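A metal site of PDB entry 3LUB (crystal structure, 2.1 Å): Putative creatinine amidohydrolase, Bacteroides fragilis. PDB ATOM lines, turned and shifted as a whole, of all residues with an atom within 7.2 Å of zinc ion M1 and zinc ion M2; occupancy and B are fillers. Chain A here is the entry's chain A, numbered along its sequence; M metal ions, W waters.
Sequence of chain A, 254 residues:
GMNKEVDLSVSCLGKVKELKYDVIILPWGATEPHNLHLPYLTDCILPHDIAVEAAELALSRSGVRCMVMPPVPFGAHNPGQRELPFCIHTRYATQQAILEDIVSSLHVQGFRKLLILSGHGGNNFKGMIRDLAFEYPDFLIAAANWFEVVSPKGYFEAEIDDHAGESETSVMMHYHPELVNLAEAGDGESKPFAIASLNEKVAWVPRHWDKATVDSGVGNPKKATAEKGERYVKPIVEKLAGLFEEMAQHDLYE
The side-chain carboxylate (OE2) of Glu 168 binds zinc ion M2, 1.9 Å away.
Water W2 is bound to zinc ion M2, at 2.0 Å.
OD1 of Asp 43 is bound to zinc ion M2, 2.0 Å away.
A ring nitrogen (NE2) of His 34 binds zinc ion M2, at 2.2 Å.
Slightly farther from zinc ion M2 lies OE1 of Glu 168 (2.8 Å).
Residues that only touch zinc ion M1: His 163.
The nearest printed residue that does not touch zinc ion M1 is His 34 (4.1 Å).
Merely in contact with zinc ion M2: His 163 and Thr 42.
Within 4 Å of zinc ion M2: His 34, Thr 42, Asp 43, His 163 and Glu 168.
The nearest printed residue that does not touch zinc ion M2 is Gly 119 (4.1 Å).
Water W2 bridges ND1 of His 163 (2.7 Å) and OE1 of Glu 168 (3.3 Å).
Water W1 bridges the side-chain carboxylate (OE2) of Glu 32 (2.7 Å) and a ring nitrogen (ND1) of His 163 (3.2 Å).
Zinc ion M1 is bound by OD2 of Asp 43 (2.2 Å), OE1 of Glu 32 (2.2 Å), ND1 of His 120 (2.4 Å) and water W2 (2.5 Å).
Slightly farther from zinc ion M1 lies water W1 (2.8 Å).
The side-chain carboxylate of Glu 168 is in hydrogen-bond range of the backbone NH of Ala 164, at 2.7 Å.
ND1 of His 34 is in hydrogen-bond range of O of Glu 32.
A ring nitrogen (ND1) of His 77 lies within hydrogen-bond range of the side-chain carboxylate (OE2) of Glu 32 (3.5 Å).
NE2 of Gln 81 lies within hydrogen-bond range of OE2 of Glu 32, 2.8 Å away.
A ring nitrogen (NE2) of His 120 sits close to a ring nitrogen (ND1) of His 77 (3.4 Å).
A ring nitrogen (NE2) of His 120 sits at hydrogen-bond distance from the backbone carbonyl oxygen (O) of Ala 76 (2.7 Å).
NE2 of His 163 sits at hydrogen-bond distance from O of Pro 33 (2.8 Å).
The backbone carbonyl oxygen (O) of Pro 39 sits at hydrogen-bond distance from the side-chain hydroxyl (OG1) of Thr 42 (2.7 Å).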
ATOM      1  N   GLY A  29      -3.069  15.276 -25.189  1.00  0.00           N
ATOM      2  CA  GLY A  29      -3.658  15.844 -24.041  1.00  0.00           C
ATOM      3  C   GLY A  29      -3.599  14.953 -22.815  1.00  0.00           C
ATOM      4  O   GLY A  29      -2.553  14.404 -22.477  1.00  0.00           O
ATOM      5  N   ALA A  30      -4.738  14.838 -22.156  1.00  0.00           N
ATOM      6  CA  ALA A  30      -4.874  14.197 -20.872  1.00  0.00           C
ATOM      7  C   ALA A  30      -6.372  14.065 -20.570  1.00  0.00           C
ATOM      8  O   ALA A  30      -7.195  14.843 -21.088  1.00  0.00           O
ATOM      9  CB  ALA A  30      -4.145  15.012 -19.794  1.00  0.00           C
ATOM     10  N   GLU A  32      -8.437  14.473 -17.310  1.00  0.00           N
ATOM     11  CA  GLU A  32      -8.001  15.167 -16.124  1.00  0.00           C
ATOM     12  C   GLU A  32      -9.034  16.206 -15.683  1.00  0.00           C
ATOM     13  O   GLU A  32      -9.408  17.050 -16.470  1.00  0.00           O
ATOM     14  CB  GLU A  32      -6.683  15.924 -16.421  1.00  0.00           C
ATOM     15  CG  GLU A  32      -6.021  16.650 -15.248  1.00  0.00           C
ATOM     16  CD  GLU A  32      -4.862  17.516 -15.693  1.00  0.00           C
ATOM     17  OE1 GLU A  32      -4.916  17.992 -16.826  1.00  0.00           O
ATOM     18  OE2 GLU A  32      -3.894  17.744 -14.920  1.00  0.00           O
ATOM     19  N   PRO A  33      -9.449  16.173 -14.419  1.00  0.00           N
ATOM     20  CA  PRO A  33     -10.244  17.256 -13.813  1.00  0.00           C
ATOM     21  C   PRO A  33      -9.629  18.659 -14.000  1.00  0.00           C
ATOM     22  O   PRO A  33      -8.442  18.870 -13.707  1.00  0.00           O
ATOM     23  CB  PRO A  33     -10.260  16.880 -12.335  1.00  0.00           C
ATOM     24  CG  PRO A  33     -10.011  15.427 -12.272  1.00  0.00           C
ATOM     25  CD  PRO A  33      -9.203  15.059 -13.474  1.00  0.00           C
ATOM     26  N   HIS A  34     -10.436  19.603 -14.457  1.00  0.00           N
ATOM     27  CA  HIS A  34     -10.029  21.012 -14.596  1.00  0.00           C
ATOM     28  C   HIS A  34     -10.913  21.961 -13.752  1.00  0.00           C
ATOM     29  O   HIS A  34     -11.881  22.550 -14.270  1.00  0.00           O
ATOM     30  CB  HIS A  34     -10.155  21.393 -16.062  1.00  0.00           C
ATOM     31  CG  HIS A  34      -8.999  20.947 -16.911  1.00  0.00           C
ATOM     32  ND1 HIS A  34      -8.746  19.628 -17.215  1.00  0.00           N
ATOM     33  CD2 HIS A  34      -8.001  21.667 -17.479  1.00  0.00           C
ATOM     34  CE1 HIS A  34      -7.662  19.553 -17.964  1.00  0.00           C
ATOM     35  NE2 HIS A  34      -7.190  20.781 -18.141  1.00  0.00           N
ATOM     36  N   LEU A  38     -14.481  22.957 -16.319  1.00  0.00           N
ATOM     37  CA  LEU A  38     -13.924  22.745 -17.667  1.00  0.00           C
ATOM     38  C   LEU A  38     -13.966  21.253 -17.951  1.00  0.00           C
ATOM     39  O   LEU A  38     -13.872  20.433 -17.034  1.00  0.00           O
ATOM     40  CB  LEU A  38     -12.505  23.287 -17.728  1.00  0.00           C
ATOM     41  CG  LEU A  38     -12.274  24.772 -18.017  1.00  0.00           C
ATOM     42  CD1 LEU A  38     -10.789  25.043 -17.763  1.00  0.00           C
ATOM     43  CD2 LEU A  38     -12.671  25.174 -19.444  1.00  0.00           C
ATOM     44  N   PRO A  39     -14.116  20.870 -19.225  1.00  0.00           N
ATOM     45  CA  PRO A  39     -14.140  19.439 -19.572  1.00  0.00           C
ATOM     46  C   PRO A  39     -12.904  18.635 -19.158  1.00  0.00           C
ATOM     47  O   PRO A  39     -11.772  19.091 -19.268  1.00  0.00           O
ATOM     48  CB  PRO A  39     -14.251  19.455 -21.103  1.00  0.00           C
ATOM     49  CG  PRO A  39     -14.842  20.743 -21.409  1.00  0.00           C
ATOM     50  CD  PRO A  39     -14.305  21.709 -20.419  1.00  0.00           C
ATOM     51  N   LEU A  41     -11.632  16.597 -20.915  1.00  0.00           N
ATOM     52  CA  LEU A  41     -10.806  16.492 -22.127  1.00  0.00           C
ATOM     53  C   LEU A  41     -10.244  17.823 -22.633  1.00  0.00           C
ATOM     54  O   LEU A  41      -9.695  17.907 -23.741  1.00  0.00           O
ATOM     55  CB  LEU A  41     -11.595  15.788 -23.242  1.00  0.00           C
ATOM     56  CG  LEU A  41     -11.894  14.266 -23.125  1.00  0.00           C
ATOM     57  CD1 LEU A  41     -12.549  13.815 -24.436  1.00  0.00           C
ATOM     58  CD2 LEU A  41     -10.653  13.401 -22.849  1.00  0.00           C
ATOM     59  N   THR A  42     -10.313  18.868 -21.816  1.00  0.00           N
ATOM     60  CA  THR A  42      -9.689  20.147 -22.175  1.00  0.00           C
ATOM     61  C   THR A  42      -8.350  20.042 -22.924  1.00  0.00           C
ATOM     62  O   THR A  42      -8.145  20.681 -23.950  1.00  0.00           O
ATOM     63  CB  THR A  42      -9.565  21.004 -20.881  1.00  0.00           C
ATOM     64  OG1 THR A  42     -10.890  21.321 -20.471  1.00  0.00           O
ATOM     65  CG2 THR A  42      -8.760  22.287 -21.087  1.00  0.00           C
ATOM     66  N   ASP A  43      -7.434  19.231 -22.388  1.00  0.00           N
ATOM     67  CA  ASP A  43      -6.068  19.184 -22.927  1.00  0.00           C
ATOM     68  C   ASP A  43      -5.969  18.474 -24.269  1.00  0.00           C
ATOM     69  O   ASP A  43      -4.942  18.561 -24.923  1.00  0.00           O
ATOM     70  CB  ASP A  43      -5.127  18.485 -21.937  1.00  0.00           C
ATOM     71  CG  ASP A  43      -4.973  19.270 -20.670  1.00  0.00           C
ATOM     72  OD1 ASP A  43      -5.484  20.403 -20.627  1.00  0.00           O
ATOM     73  OD2 ASP A  43      -4.366  18.757 -19.727  1.00  0.00           O
ATOM     74  N   CYS A  44      -7.017  17.749 -24.640  1.00  0.00           N
ATOM     75  CA  CYS A  44      -7.145  17.208 -25.966  1.00  0.00           C
ATOM     76  C   CYS A  44      -7.813  18.209 -26.911  1.00  0.00           C
ATOM     77  O   CYS A  44      -7.396  18.391 -28.063  1.00  0.00           O
ATOM     78  CB  CYS A  44      -8.000  15.943 -25.931  1.00  0.00           C
ATOM     79  SG  CYS A  44      -7.224  14.552 -25.148  1.00  0.00           S
ATOM     80  N   LEU A  46      -8.336  21.550 -26.834  1.00  0.00           N
ATOM     81  CA  LEU A  46      -7.657  22.803 -27.176  1.00  0.00           C
ATOM     82  C   LEU A  46      -6.517  22.670 -28.195  1.00  0.00           C
ATOM     83  O   LEU A  46      -6.502  23.414 -29.169  1.00  0.00           O
ATOM     84  CB  LEU A  46      -7.240  23.593 -25.920  1.00  0.00           C
ATOM     85  CG  LEU A  46      -8.399  24.040 -25.010  1.00  0.00           C
ATOM     86  CD1 LEU A  46      -7.867  24.925 -23.867  1.00  0.00           C
ATOM     87  CD2 LEU A  46      -9.561  24.772 -25.751  1.00  0.00           C
ATOM     88  N   ALA A  76       0.407  12.386 -18.311  1.00  0.00           N
ATOM     89  CA  ALA A  76       1.233  12.028 -17.167  1.00  0.00           C
ATOM     90  C   ALA A  76       0.844  12.953 -16.030  1.00  0.00           C
ATOM     91  O   ALA A  76       0.884  14.168 -16.188  1.00  0.00           O
ATOM     92  CB  ALA A  76       2.720  12.215 -17.550  1.00  0.00           C
ATOM     93  N   HIS A  77       0.431  12.386 -14.901  1.00  0.00           N
ATOM     94  CA  HIS A  77      -0.150  13.184 -13.793  1.00  0.00           C
ATOM     95  C   HIS A  77       0.652  13.104 -12.505  1.00  0.00           C
ATOM     96  O   HIS A  77       1.627  12.347 -12.406  1.00  0.00           O
ATOM     97  CB  HIS A  77      -1.632  12.830 -13.570  1.00  0.00           C
ATOM     98  CG  HIS A  77      -2.476  13.172 -14.749  1.00  0.00           C
ATOM     99  ND1 HIS A  77      -2.691  14.478 -15.141  1.00  0.00           N
ATOM    100  CD2 HIS A  77      -3.007  12.392 -15.724  1.00  0.00           C
ATOM    101  CE1 HIS A  77      -3.374  14.479 -16.275  1.00  0.00           C
ATOM    102  NE2 HIS A  77      -3.572  13.221 -16.645  1.00  0.00           N
ATOM    103  N   GLN A  81      -3.695  13.499  -8.055  1.00  0.00           N
ATOM    104  CA  GLN A  81      -4.593  13.614  -9.195  1.00  0.00           C
ATOM    105  C   GLN A  81      -5.234  12.265  -9.573  1.00  0.00           C
ATOM    106  O   GLN A  81      -6.383  12.228 -10.018  1.00  0.00           O
ATOM    107  CB  GLN A  81      -3.853  14.117 -10.416  1.00  0.00           C
ATOM    108  CG  GLN A  81      -3.354  15.538 -10.334  1.00  0.00           C
ATOM    109  CD  GLN A  81      -2.985  16.052 -11.709  1.00  0.00           C
ATOM    110  OE1 GLN A  81      -1.879  15.842 -12.199  1.00  0.00           O
ATOM    111  NE2 GLN A  81      -3.939  16.734 -12.347  1.00  0.00           N
ATOM    112  N   GLY A 119      -1.250  19.658 -24.960  1.00  0.00           N
ATOM    113  CA  GLY A 119      -2.152  20.448 -24.189  1.00  0.00           C
ATOM    114  C   GLY A 119      -1.953  20.281 -22.714  1.00  0.00           C
ATOM    115  O   GLY A 119      -2.596  20.973 -21.956  1.00  0.00           O
ATOM    116  N   HIS A 120      -1.048  19.392 -22.308  1.00  0.00           N
ATOM    117  CA  HIS A 120      -0.828  19.038 -20.913  1.00  0.00           C
ATOM    118  C   HIS A 120       0.664  19.194 -20.584  1.00  0.00           C
ATOM    119  O   HIS A 120       1.551  18.528 -21.163  1.00  0.00           O
ATOM    120  CB  HIS A 120      -1.296  17.606 -20.653  1.00  0.00           C
ATOM    121  CG  HIS A 120      -1.089  17.113 -19.248  1.00  0.00           C
ATOM    122  ND1 HIS A 120      -1.617  17.742 -18.151  1.00  0.00           N
ATOM    123  CD2 HIS A 120      -0.453  16.004 -18.780  1.00  0.00           C
ATOM    124  CE1 HIS A 120      -1.312  17.057 -17.055  1.00  0.00           C
ATOM    125  NE2 HIS A 120      -0.601  16.004 -17.405  1.00  0.00           N
ATOM    126  N   GLY A 121       0.944  20.107 -19.659  1.00  0.00           N
ATOM    127  CA  GLY A 121       2.325  20.407 -19.312  1.00  0.00           C
ATOM    128  C   GLY A 121       3.007  19.289 -18.571  1.00  0.00           C
ATOM    129  O   GLY A 121       4.215  19.268 -18.510  1.00  0.00           O
ATOM    130  N   GLY A 122       2.227  18.380 -17.988  1.00  0.00           N
ATOM    131  CA  GLY A 122       2.753  17.153 -17.372  1.00  0.00           C
ATOM    132  C   GLY A 122       3.443  16.241 -18.356  1.00  0.00           C
ATOM    133  O   GLY A 122       4.265  15.412 -17.968  1.00  0.00           O
ATOM    134  N   TRP A 146       0.960  24.014 -26.673  1.00  0.00           N
ATOM    135  CA  TRP A 146       0.252  25.103 -27.335  1.00  0.00           C
ATOM    136  C   TRP A 146       0.342  26.414 -26.552  1.00  0.00           C
ATOM    137  O   TRP A 146       0.506  27.466 -27.150  1.00  0.00           O
ATOM    138  CB  TRP A 146      -1.239  24.737 -27.706  1.00  0.00           C
ATOM    139  CG  TRP A 146      -2.175  24.700 -26.552  1.00  0.00           C
ATOM    140  CD1 TRP A 146      -2.563  23.600 -25.865  1.00  0.00           C
ATOM    141  CD2 TRP A 146      -2.864  25.821 -25.943  1.00  0.00           C
ATOM    142  NE1 TRP A 146      -3.430  23.951 -24.875  1.00  0.00           N
ATOM    143  CE2 TRP A 146      -3.620  25.308 -24.881  1.00  0.00           C
ATOM    144  CE3 TRP A 146      -2.875  27.219 -26.184  1.00  0.00           C
ATOM    145  CZ2 TRP A 146      -4.417  26.137 -24.054  1.00  0.00           C
ATOM    146  CZ3 TRP A 146      -3.670  28.033 -25.376  1.00  0.00           C
ATOM    147  CH2 TRP A 146      -4.445  27.489 -24.317  1.00  0.00           C
ATOM    148  N   PHE A 147       0.285  26.322 -25.226  1.00  0.00           N
ATOM    149  CA  PHE A 147       0.261  27.493 -24.336  1.00  0.00           C
ATOM    150  C   PHE A 147       1.615  28.147 -24.051  1.00  0.00           C
ATOM    151  O   PHE A 147       1.684  29.121 -23.283  1.00  0.00           O
ATOM    152  CB  PHE A 147      -0.406  27.129 -22.984  1.00  0.00           C
ATOM    153  CG  PHE A 147       0.156  25.896 -22.368  1.00  0.00           C
ATOM    154  CD1 PHE A 147       1.291  25.960 -21.566  1.00  0.00           C
ATOM    155  CD2 PHE A 147      -0.419  24.666 -22.594  1.00  0.00           C
ATOM    156  CE1 PHE A 147       1.816  24.831 -21.012  1.00  0.00           C
ATOM    157  CE2 PHE A 147       0.118  23.510 -22.034  1.00  0.00           C
ATOM    158  CZ  PHE A 147       1.228  23.591 -21.261  1.00  0.00           C
ATOM    159  N   ASP A 162      -2.073  28.252 -13.783  1.00  0.00           N
ATOM    160  CA  ASP A 162      -1.269  27.061 -14.136  1.00  0.00           C
ATOM    161  C   ASP A 162      -2.124  25.900 -14.694  1.00  0.00           C
ATOM    162  O   ASP A 162      -1.655  25.105 -15.509  1.00  0.00           O
ATOM    163  CB  ASP A 162      -0.488  26.568 -12.897  1.00  0.00           C
ATOM    164  CG  ASP A 162       0.766  27.408 -12.584  1.00  0.00           C
ATOM    165  OD1 ASP A 162       1.231  28.166 -13.457  1.00  0.00           O
ATOM    166  OD2 ASP A 162       1.325  27.301 -11.474  1.00  0.00           O
ATOM    167  N   HIS A 163      -3.363  25.768 -14.217  1.00  0.00           N
ATOM    168  CA  HIS A 163      -4.221  24.661 -14.625  1.00  0.00           C
ATOM    169  C   HIS A 163      -5.674  25.016 -14.441  1.00  0.00           C
ATOM    170  O   HIS A 163      -6.138  25.158 -13.301  1.00  0.00           O
ATOM    171  CB  HIS A 163      -3.935  23.435 -13.763  1.00  0.00           C
ATOM    172  CG  HIS A 163      -4.873  22.289 -14.033  1.00  0.00           C
ATOM    173  ND1 HIS A 163      -4.895  21.614 -15.223  1.00  0.00           N
ATOM    174  CD2 HIS A 163      -5.802  21.695 -13.239  1.00  0.00           C
ATOM    175  CE1 HIS A 163      -5.807  20.654 -15.160  1.00  0.00           C
ATOM    176  NE2 HIS A 163      -6.371  20.681 -13.974  1.00  0.00           N
ATOM    177  N   ALA A 164      -6.376  25.121 -15.569  1.00  0.00           N
ATOM    178  CA  ALA A 164      -7.832  25.395 -15.597  1.00  0.00           C
ATOM    179  C   ALA A 164      -8.152  26.828 -15.093  1.00  0.00           C
ATOM    180  O   ALA A 164      -9.234  27.112 -14.572  1.00  0.00           O
ATOM    181  CB  ALA A 164      -8.578  24.369 -14.805  1.00  0.00           C
ATOM    182  N   GLU A 168      -6.790  28.865 -19.894  1.00  0.00           N
ATOM    183  CA  GLU A 168      -7.474  27.689 -20.467  1.00  0.00           C
ATOM    184  C   GLU A 168      -8.977  27.912 -20.627  1.00  0.00           C
ATOM    185  O   GLU A 168      -9.572  27.477 -21.632  1.00  0.00           O
ATOM    186  CB  GLU A 168      -7.247  26.409 -19.626  1.00  0.00           C
ATOM    187  CG  GLU A 168      -6.091  25.559 -20.124  1.00  0.00           C
ATOM    188  CD  GLU A 168      -5.896  24.253 -19.383  1.00  0.00           C
ATOM    189  OE1 GLU A 168      -6.088  24.194 -18.139  1.00  0.00           O
ATOM    190  OE2 GLU A 168      -5.500  23.266 -20.054  1.00  0.00           O
ATOM    191  N   TRP A 209      -1.538  17.396  -5.740  1.00  0.00           N
ATOM    192  CA  TRP A 209      -2.886  18.006  -5.885  1.00  0.00           C
ATOM    193  C   TRP A 209      -3.725  17.905  -4.616  1.00  0.00           C
ATOM    194  O   TRP A 209      -4.525  18.818  -4.318  1.00  0.00           O
ATOM    195  CB  TRP A 209      -3.677  17.363  -7.028  1.00  0.00           C
ATOM    196  CG  TRP A 209      -3.926  18.253  -8.170  1.00  0.00           C
ATOM    197  CD1 TRP A 209      -5.122  18.749  -8.586  1.00  0.00           C
ATOM    198  CD2 TRP A 209      -2.948  18.755  -9.076  1.00  0.00           C
ATOM    199  NE1 TRP A 209      -4.957  19.531  -9.699  1.00  0.00           N
ATOM    200  CE2 TRP A 209      -3.630  19.557 -10.027  1.00  0.00           C
ATOM    201  CE3 TRP A 209      -1.550  18.613  -9.192  1.00  0.00           C
ATOM    202  CZ2 TRP A 209      -2.965  20.222 -11.075  1.00  0.00           C
ATOM    203  CZ3 TRP A 209      -0.903  19.262 -10.223  1.00  0.00           C
ATOM    204  CH2 TRP A 209      -1.608  20.058 -11.158  1.00  0.00           C
HETATM  205 ZN    ZN M   1      -3.392  19.284 -17.815  1.00  0.00          ZN
HETATM  206 ZN    ZN M   2      -5.428  21.659 -19.057  1.00  0.00          ZN
HETATM  207  O   HOH W   1      -2.230  19.864 -15.285  1.00  0.00           O
HETATM  208  O   HOH W   2      -3.930  21.738 -17.720  1.00  0.00           O
HETATM  209  O   HOH W   3      -1.361  21.558 -18.439  1.00  0.00           O
